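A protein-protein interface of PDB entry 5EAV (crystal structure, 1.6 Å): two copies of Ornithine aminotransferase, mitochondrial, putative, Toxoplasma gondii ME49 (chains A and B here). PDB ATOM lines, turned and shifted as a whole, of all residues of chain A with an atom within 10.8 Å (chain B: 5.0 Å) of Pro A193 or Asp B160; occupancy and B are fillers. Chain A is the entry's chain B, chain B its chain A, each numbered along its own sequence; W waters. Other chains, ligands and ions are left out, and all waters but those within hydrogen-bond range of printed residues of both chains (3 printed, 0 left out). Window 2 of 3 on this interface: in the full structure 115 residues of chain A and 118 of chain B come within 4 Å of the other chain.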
ATOM      1  N   THR A 175      13.044  15.138   6.746  1.00  0.00           N
ATOM      2  CA  THR A 175      12.970  16.538   6.715  1.00  0.00           C
ATOM      3  C   THR A 175      11.740  16.986   7.509  1.00  0.00           C
ATOM      4  O   THR A 175      10.884  16.165   7.829  1.00  0.00           O
ATOM      5  CB  THR A 175      12.795  17.050   5.288  1.00  0.00           C
ATOM      6  OG1 THR A 175      11.624  16.524   4.711  1.00  0.00           O
ATOM      7  CG2 THR A 175      14.027  16.655   4.433  1.00  0.00           C
ATOM      8  N   ILE A 176      11.623  18.285   7.786  1.00  0.00           N
ATOM      9  CA  ILE A 176      10.442  18.733   8.515  1.00  0.00           C
ATOM     10  C   ILE A 176       9.134  18.431   7.746  1.00  0.00           C
ATOM     11  O   ILE A 176       8.103  18.065   8.365  1.00  0.00           O
ATOM     12  CB  ILE A 176      10.580  20.204   8.967  1.00  0.00           C
ATOM     13  CG1 ILE A 176      11.649  20.238  10.076  1.00  0.00           C
ATOM     14  CG2 ILE A 176       9.233  20.800   9.459  1.00  0.00           C
ATOM     15  CD1 ILE A 176      12.149  21.618  10.459  1.00  0.00           C
ATOM     16  N   THR A 177       9.158  18.610   6.419  1.00  0.00           N
ATOM     17  CA  THR A 177       7.977  18.300   5.638  1.00  0.00           C
ATOM     18  C   THR A 177       7.607  16.816   5.667  1.00  0.00           C
ATOM     19  O   THR A 177       6.423  16.460   5.711  1.00  0.00           O
ATOM     20  CB  THR A 177       8.073  18.928   4.243  1.00  0.00           C
ATOM     21  OG1 THR A 177       8.194  20.336   4.397  1.00  0.00           O
ATOM     22  CG2 THR A 177       6.810  18.613   3.445  1.00  0.00           C
ATOM     23  N   ALA A 178       8.601  15.927   5.750  1.00  0.00           N
ATOM     24  CA  ALA A 178       8.311  14.521   5.850  1.00  0.00           C
ATOM     25  C   ALA A 178       7.740  14.275   7.229  1.00  0.00           C
ATOM     26  O   ALA A 178       6.773  13.591   7.350  1.00  0.00           O
ATOM     27  CB  ALA A 178       9.563  13.694   5.587  1.00  0.00           C
ATOM     28  N   CYS A 179       8.328  14.858   8.278  1.00  0.00           N
ATOM     29  CA  CYS A 179       7.770  14.727   9.638  1.00  0.00           C
ATOM     30  C   CYS A 179       6.339  15.233   9.681  1.00  0.00           C
ATOM     31  O   CYS A 179       5.497  14.661  10.357  1.00  0.00           O
ATOM     32  CB  CYS A 179       8.598  15.524  10.667  1.00  0.00           C
ATOM     33  SG  CYS A 179      10.297  14.944  10.774  1.00  0.00           S
ATOM     34  N   SER A 180       6.037  16.253   8.881  1.00  0.00           N
ATOM     35  CA  SER A 180       4.716  16.835   8.878  1.00  0.00           C
ATOM     36  C   SER A 180       3.678  15.946   8.201  1.00  0.00           C
ATOM     37  O   SER A 180       2.484  16.140   8.391  1.00  0.00           O
ATOM     38  CB  SER A 180       4.758  18.154   8.116  1.00  0.00           C
ATOM     39  OG  SER A 180       5.670  19.060   8.696  1.00  0.00           O
ATOM     40  N   SER A 181       4.131  14.959   7.447  1.00  0.00           N
ATOM     41  CA  SER A 181       3.245  14.028   6.736  1.00  0.00           C
ATOM     42  C   SER A 181       3.326  12.599   7.291  1.00  0.00           C
ATOM     43  O   SER A 181       2.802  11.674   6.695  1.00  0.00           O
ATOM     44  CB  SER A 181       3.565  14.053   5.251  1.00  0.00           C
ATOM     45  OG  SER A 181       4.902  13.787   4.975  1.00  0.00           O
ATOM     46  N   CYS A 187       8.775  10.183  14.748  1.00  0.00           N
ATOM     47  CA  CYS A 187       9.186  10.915  13.567  1.00  0.00           C
ATOM     48  C   CYS A 187       8.748  12.375  13.615  1.00  0.00           C
ATOM     49  O   CYS A 187       9.430  13.222  13.064  1.00  0.00           O
ATOM     50  CB  CYS A 187       8.603  10.275  12.314  1.00  0.00           C
ATOM     51  SG  CYS A 187       9.348  10.883  10.784  1.00  0.00           S
ATOM     52  N   TYR A 188       7.582  12.660  14.198  1.00  0.00           N
ATOM     53  CA  TYR A 188       7.081  14.045  14.268  1.00  0.00           C
ATOM     54  C   TYR A 188       7.125  14.727  15.618  1.00  0.00           C
ATOM     55  O   TYR A 188       7.207  15.940  15.666  1.00  0.00           O
ATOM     56  CB  TYR A 188       5.660  14.194  13.723  1.00  0.00           C
ATOM     57  CG  TYR A 188       4.576  13.523  14.511  1.00  0.00           C
ATOM     58  CD1 TYR A 188       4.064  14.080  15.678  1.00  0.00           C
ATOM     59  CD2 TYR A 188       4.056  12.316  14.087  1.00  0.00           C
ATOM     60  CE1 TYR A 188       3.067  13.440  16.404  1.00  0.00           C
ATOM     61  CE2 TYR A 188       3.078  11.656  14.823  1.00  0.00           C
ATOM     62  CZ  TYR A 188       2.566  12.220  15.973  1.00  0.00           C
ATOM     63  OH  TYR A 188       1.563  11.554  16.728  1.00  0.00           O
ATOM     64  N   ASN A 189       7.206  13.974  16.718  1.00  0.00           N
ATOM     65  CA  ASN A 189       7.010  14.608  18.008  1.00  0.00           C
ATOM     66  C   ASN A 189       8.026  15.682  18.315  1.00  0.00           C
ATOM     67  O   ASN A 189       9.217  15.466  18.202  1.00  0.00           O
ATOM     68  CB  ASN A 189       7.045  13.584  19.121  1.00  0.00           C
ATOM     69  CG  ASN A 189       6.800  14.201  20.498  1.00  0.00           C
ATOM     70  OD1 ASN A 189       5.833  14.917  20.704  1.00  0.00           O
ATOM     71  ND2 ASN A 189       7.673  13.896  21.437  1.00  0.00           N
ATOM     72  N   ASN A 190       7.506  16.846  18.683  1.00  0.00           N
ATOM     73  CA  ASN A 190       8.347  17.987  19.018  1.00  0.00           C
ATOM     74  C   ASN A 190       9.230  18.557  17.907  1.00  0.00           C
ATOM     75  O   ASN A 190      10.220  19.267  18.191  1.00  0.00           O
ATOM     76  CB  ASN A 190       9.156  17.700  20.294  1.00  0.00           C
ATOM     77  CG  ASN A 190       8.341  17.883  21.539  1.00  0.00           C
ATOM     78  OD1 ASN A 190       7.319  18.565  21.527  1.00  0.00           O
ATOM     79  ND2 ASN A 190       8.843  17.357  22.647  1.00  0.00           N
ATOM     80  N   PHE A 191       8.785  18.378  16.654  1.00  0.00           N
ATOM     81  CA  PHE A 191       9.507  18.929  15.528  1.00  0.00           C
ATOM     82  C   PHE A 191       8.624  19.941  14.781  1.00  0.00           C
ATOM     83  O   PHE A 191       9.083  20.478  13.782  1.00  0.00           O
ATOM     84  CB  PHE A 191       9.997  17.818  14.585  1.00  0.00           C
ATOM     85  CG  PHE A 191      11.058  16.916  15.188  1.00  0.00           C
ATOM     86  CD1 PHE A 191      12.241  17.426  15.668  1.00  0.00           C
ATOM     87  CD2 PHE A 191      10.946  15.550  15.047  1.00  0.00           C
ATOM     88  CE1 PHE A 191      13.230  16.595  16.197  1.00  0.00           C
ATOM     89  CE2 PHE A 191      11.937  14.709  15.556  1.00  0.00           C
ATOM     90  CZ  PHE A 191      13.094  15.233  16.096  1.00  0.00           C
ATOM     91  N   GLY A 192       7.434  20.262  15.313  1.00  0.00           N
ATOM     92  CA  GLY A 192       6.517  21.287  14.642  1.00  0.00           C
ATOM     93  C   GLY A 192       6.943  22.727  14.939  1.00  0.00           C
ATOM     94  O   GLY A 192       7.864  22.944  15.703  1.00  0.00           O
ATOM     95  N   PRO A 193       6.238  23.741  14.425  1.00  0.00           N
ATOM     96  CA  PRO A 193       5.010  23.561  13.661  1.00  0.00           C
ATOM     97  C   PRO A 193       5.242  22.887  12.302  1.00  0.00           C
ATOM     98  O   PRO A 193       6.334  22.977  11.719  1.00  0.00           O
ATOM     99  CB  PRO A 193       4.460  24.979  13.563  1.00  0.00           C
ATOM    100  CG  PRO A 193       5.659  25.856  13.624  1.00  0.00           C
ATOM    101  CD  PRO A 193       6.586  25.158  14.597  1.00  0.00           C
ATOM    102  N   PHE A 194       4.202  22.242  11.823  1.00  0.00           N
ATOM    103  CA  PHE A 194       4.290  21.415  10.636  1.00  0.00           C
ATOM    104  C   PHE A 194       3.804  22.033   9.350  1.00  0.00           C
ATOM    105  O   PHE A 194       2.992  22.969   9.328  1.00  0.00           O
ATOM    106  CB  PHE A 194       3.534  20.128  10.900  1.00  0.00           C
ATOM    107  CG  PHE A 194       4.037  19.382  12.124  1.00  0.00           C
ATOM    108  CD1 PHE A 194       5.238  18.754  12.074  1.00  0.00           C
ATOM    109  CD2 PHE A 194       3.291  19.316  13.317  1.00  0.00           C
ATOM    110  CE1 PHE A 194       5.744  18.073  13.200  1.00  0.00           C
ATOM    111  CE2 PHE A 194       3.802  18.652  14.458  1.00  0.00           C
ATOM    112  CZ  PHE A 194       5.013  18.022  14.375  1.00  0.00           C
ATOM    113  N   THR A 195       4.391  21.525   8.265  1.00  0.00           N
ATOM    114  CA  THR A 195       3.992  21.971   6.944  1.00  0.00           C
ATOM    115  C   THR A 195       2.559  21.532   6.715  1.00  0.00           C
ATOM    116  O   THR A 195       2.226  20.358   6.921  1.00  0.00           O
ATOM    117  CB  THR A 195       4.879  21.282   5.866  1.00  0.00           C
ATOM    118  OG1 THR A 195       6.260  21.475   6.175  1.00  0.00           O
ATOM    119  CG2 THR A 195       4.577  21.834   4.485  1.00  0.00           C
ATOM    120  N   PRO A 196       1.668  22.469   6.284  1.00  0.00           N
ATOM    121  CA  PRO A 196       0.299  22.004   5.998  1.00  0.00           C
ATOM    122  C   PRO A 196       0.197  21.404   4.597  1.00  0.00           C
ATOM    123  O   PRO A 196       1.182  21.393   3.835  1.00  0.00           O
ATOM    124  CB  PRO A 196      -0.536  23.274   6.048  1.00  0.00           C
ATOM    125  CG  PRO A 196       0.410  24.379   5.902  1.00  0.00           C
ATOM    126  CD  PRO A 196       1.773  23.931   6.312  1.00  0.00           C
ATOM    127  N   GLY A 197      -0.997  20.929   4.275  1.00  0.00           N
ATOM    128  CA  GLY A 197      -1.279  20.408   2.954  1.00  0.00           C
ATOM    129  C   GLY A 197      -1.271  18.912   2.715  1.00  0.00           C
ATOM    130  O   GLY A 197      -1.275  18.479   1.562  1.00  0.00           O
ATOM    131  N   PHE A 198      -1.393  18.124   3.789  1.00  0.00           N
ATOM    132  CA  PHE A 198      -1.419  16.705   3.657  1.00  0.00           C
ATOM    133  C   PHE A 198      -2.713  16.097   4.185  1.00  0.00           C
ATOM    134  O   PHE A 198      -3.248  16.546   5.201  1.00  0.00           O
ATOM    135  CB  PHE A 198      -0.198  16.112   4.398  1.00  0.00           C
ATOM    136  CG  PHE A 198       1.105  16.658   3.868  1.00  0.00           C
ATOM    137  CD1 PHE A 198       1.599  16.194   2.658  1.00  0.00           C
ATOM    138  CD2 PHE A 198       1.754  17.726   4.467  1.00  0.00           C
ATOM    139  CE1 PHE A 198       2.753  16.702   2.098  1.00  0.00           C
ATOM    140  CE2 PHE A 198       2.912  18.247   3.923  1.00  0.00           C
ATOM    141  CZ  PHE A 198       3.422  17.731   2.737  1.00  0.00           C
ATOM    142  N   ARG B 148      14.243  23.096  17.478  1.00  0.00           N
ATOM    143  CA  ARG B 148      12.826  23.024  17.872  1.00  0.00           C
ATOM    144  C   ARG B 148      12.623  22.107  19.049  1.00  0.00           C
ATOM    145  O   ARG B 148      11.979  22.511  20.045  1.00  0.00           O
ATOM    146  CB  ARG B 148      11.935  22.608  16.704  1.00  0.00           C
ATOM    147  CG  ARG B 148      11.670  23.707  15.706  1.00  0.00           C
ATOM    148  CD  ARG B 148      10.976  23.189  14.493  1.00  0.00           C
ATOM    149  NE  ARG B 148      10.495  24.288  13.646  1.00  0.00           N
ATOM    150  CZ  ARG B 148       9.583  24.160  12.708  1.00  0.00           C
ATOM    151  NH1 ARG B 148       9.041  22.979  12.417  1.00  0.00           N
ATOM    152  NH2 ARG B 148       9.189  25.248  12.062  1.00  0.00           N
ATOM    153  N   TYR B 152      11.365  22.961  22.816  1.00  0.00           N
ATOM    154  CA  TYR B 152      10.202  22.376  23.472  1.00  0.00           C
ATOM    155  C   TYR B 152      10.528  21.656  24.787  1.00  0.00           C
ATOM    156  O   TYR B 152       9.790  21.795  25.758  1.00  0.00           O
ATOM    157  CB  TYR B 152       9.466  21.416  22.571  1.00  0.00           C
ATOM    158  CG  TYR B 152       8.885  22.126  21.340  1.00  0.00           C
ATOM    159  CD1 TYR B 152       8.143  23.275  21.487  1.00  0.00           C
ATOM    160  CD2 TYR B 152       9.061  21.628  20.071  1.00  0.00           C
ATOM    161  CE1 TYR B 152       7.655  23.958  20.387  1.00  0.00           C
ATOM    162  CE2 TYR B 152       8.548  22.300  18.952  1.00  0.00           C
ATOM    163  CZ  TYR B 152       7.836  23.460  19.124  1.00  0.00           C
ATOM    164  OH  TYR B 152       7.286  24.191  18.057  1.00  0.00           O
ATOM    165  N   PRO B 158       5.768  26.758  24.696  1.00  0.00           N
ATOM    166  CA  PRO B 158       4.522  26.053  24.378  1.00  0.00           C
ATOM    167  C   PRO B 158       4.547  25.150  23.108  1.00  0.00           C
ATOM    168  O   PRO B 158       5.252  25.460  22.156  1.00  0.00           O
ATOM    169  CB  PRO B 158       3.494  27.183  24.227  1.00  0.00           C
ATOM    170  CG  PRO B 158       4.099  28.397  24.840  1.00  0.00           C
ATOM    171  CD  PRO B 158       5.585  28.216  24.837  1.00  0.00           C
ATOM    172  N   PRO B 159       3.739  24.075  23.079  1.00  0.00           N
ATOM    173  CA  PRO B 159       3.782  23.197  21.919  1.00  0.00           C
ATOM    174  C   PRO B 159       3.477  23.920  20.612  1.00  0.00           C
ATOM    175  O   PRO B 159       2.636  24.831  20.574  1.00  0.00           O
ATOM    176  CB  PRO B 159       2.730  22.111  22.235  1.00  0.00           C
ATOM    177  CG  PRO B 159       2.309  22.341  23.659  1.00  0.00           C
ATOM    178  CD  PRO B 159       2.573  23.785  23.943  1.00  0.00           C
ATOM    179  N   ASP B 160       4.225  23.544  19.566  1.00  0.00           N
ATOM    180  CA  ASP B 160       4.121  24.134  18.239  1.00  0.00           C
ATOM    181  C   ASP B 160       4.381  25.629  18.103  1.00  0.00           C
ATOM    182  O   ASP B 160       4.174  26.163  17.020  1.00  0.00           O
ATOM    183  CB  ASP B 160       2.800  23.735  17.536  1.00  0.00           C
ATOM    184  CG  ASP B 160       2.879  22.348  16.879  1.00  0.00           C
ATOM    185  OD1 ASP B 160       3.987  21.835  16.651  1.00  0.00           O
ATOM    186  OD2 ASP B 160       1.840  21.770  16.560  1.00  0.00           O
ATOM    187  N   SER B 161       4.911  26.287  19.141  1.00  0.00           N
ATOM    188  CA  SER B 161       5.117  27.746  19.107  1.00  0.00           C
ATOM    189  C   SER B 161       6.531  28.156  18.761  1.00  0.00           C
ATOM    190  O   SER B 161       6.790  29.376  18.657  1.00  0.00           O
ATOM    191  CB  SER B 161       4.804  28.383  20.473  1.00  0.00           C
ATOM    192  OG  SER B 161       5.832  28.087  21.431  1.00  0.00           O
ATOM    193  N   ALA B 162       7.444  27.176  18.600  1.00  0.00           N
ATOM    194  CA  ALA B 162       8.844  27.492  18.311  1.00  0.00           C
ATOM    195  C   ALA B 162       9.010  28.356  17.064  1.00  0.00           C
ATOM    196  O   ALA B 162       8.378  28.092  16.008  1.00  0.00           O
ATOM    197  CB  ALA B 162       9.649  26.232  18.135  1.00  0.00           C
ATOM    198  N   THR B 195       5.807  25.773   5.594  1.00  0.00           N
ATOM    199  CA  THR B 195       6.032  25.480   6.962  1.00  0.00           C
ATOM    200  C   THR B 195       6.036  26.805   7.785  1.00  0.00           C
ATOM    201  O   THR B 195       6.790  27.728   7.486  1.00  0.00           O
ATOM    202  CB  THR B 195       7.413  24.841   7.133  1.00  0.00           C
ATOM    203  OG1 THR B 195       7.579  23.754   6.196  1.00  0.00           O
ATOM    204  CG2 THR B 195       7.586  24.372   8.547  1.00  0.00           C
ATOM    205  N   PRO B 196       5.171  26.910   8.784  1.00  0.00           N
ATOM    206  CA  PRO B 196       5.198  28.095   9.647  1.00  0.00           C
ATOM    207  C   PRO B 196       6.381  28.080  10.632  1.00  0.00           C
ATOM    208  O   PRO B 196       7.147  27.141  10.682  1.00  0.00           O
ATOM    209  CB  PRO B 196       3.916  27.964  10.489  1.00  0.00           C
ATOM    210  CG  PRO B 196       3.277  26.678  10.107  1.00  0.00           C
ATOM    211  CD  PRO B 196       4.202  25.909   9.237  1.00  0.00           C
ATOM    212  N   GLY B 197       6.501  29.153  11.403  1.00  0.00           N
ATOM    213  CA  GLY B 197       7.521  29.251  12.454  1.00  0.00           C
ATOM    214  C   GLY B 197       8.803  30.005  12.130  1.00  0.00           C
ATOM    215  O   GLY B 197       9.793  29.855  12.864  1.00  0.00           O
HETATM  216  O   HOH W   1       5.641  21.134  19.978  1.00  0.00           O
HETATM  217  O   HOH W   2       1.795  22.407  13.525  1.00  0.00           O
HETATM  218  O   HOH W   3       5.662  20.216  17.399  1.00  0.00           O
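The guanidinium group (NH1) of Arg B148 is in hydrogen-bond range of the backbone carbonyl oxygen (O) of Phe A191. The guanidinium group of Arg B148 sits close to the backbone carbonyl oxygen of Gly A192, at 3.5 Å. O of Pro A193 sits at hydrogen-bond distance from NH1 of Arg B148 (2.8 Å). The backbone carbonyl oxygen (O) of Gly A192 lies within hydrogen-bond range of the side-chain hydroxyl (OH) of Tyr B152 (2.7 Å). OG1 of Thr A195 sits at hydrogen-bond distance from OG1 of Thr B195 (2.6 Å).
N of Asp B160 lies close to OH of Tyr B152, at 3.5 Å. The side-chain hydroxyl of Tyr B152 is in hydrogen-bond range of the backbone NH of Ser B161 (3.3 Å). OH of Tyr B152 sits at hydrogen-bond distance from N of Ala B162 (3.0 Å). The backbone carbonyl oxygen (O) of Ile A176 sits at hydrogen-bond distance from the side-chain hydroxyl (OG) of Ser A180, 2.6 Å away. OG1 of Thr A177 sits at hydrogen-bond distance from OG1 of Thr A195 (2.9 Å). The side-chain hydroxyl (OG) of Ser A180 sits at hydrogen-bond distance from the backbone NH (N) of Thr A195 (2.8 Å).
Among the printed residues, merely in contact across the chains: Phe A194 with Pro B196, Asn A190 with Tyr B152, Gly A192 with Asp B160, Pro A193 with Pro B196, Pro A193 with Asp B160, Pro A193 with Tyr B152, Ile A176 with Arg B148, Pro A193 with Thr B195, Pro A193 with Ala B162, Asn A190 with Arg B148, Phe A194 with Asp B160 and Thr A177 with Thr B195.
Of chain B, only Arg B148, Tyr B152, Asp B160, Ala B162, Thr B195 and Pro B196 come within 4 Å of Pro A193. Of chain A, only Gly A192, Pro A193 and Phe A194 come within 4 Å of Asp B160. No residue of chain A comes within 4 Å of Ser B161. Of chain A, only Pro A193 (3.7 Å) comes within 4 Å of Ala B162. Of the printed residues of chain A, Tyr B152 touches Asn A190, Gly A192 and Pro A193. Of the printed residues of chain B, Thr A195 touches Thr B195 (2.6 Å). Thr A175 touches none of the printed residues of chain B. Ala A178 touches none of the printed residues of chain B. The nearest residue of chain B that does not touch Pro A193 is Gly B197 (4.04 Å). The nearest residue of chain A that does not touch Asp B160 is Phe A191 (5.3 Å). The nearest printed residue of chain A that does not touch Thr B195 is Ile A176 (4.04 Å).
Of the 10 printed residues of chain B, 6 touch a printed residue of chain A. Printed residues of chain B that touch a printed residue of chain A: Arg B148, Tyr B152, Asp B160, Ala B162, Thr B195 and Pro B196. Along chain B the printed residues that touch a printed residue of chain A span positions 148 to 196. Among the printed residues, 17 pairs touch across the chains.
Thr B195 touches its own counterpart, Thr A195. 3 positions are printed for both chains.
Water W3 bridges OD1 of Asp B160 and N of Gly A192. Water W1 bridges the backbone NH of Asp B160 (2.8 Å) and the side-chain amide oxygen of Asn A190 (3.4 Å). Water W2 lies within hydrogen-bond range of the backbone NH (N) of Phe A194 (3.0 Å) and the side-chain carboxylate (OD2) of Asp B160 (3.1 Å).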
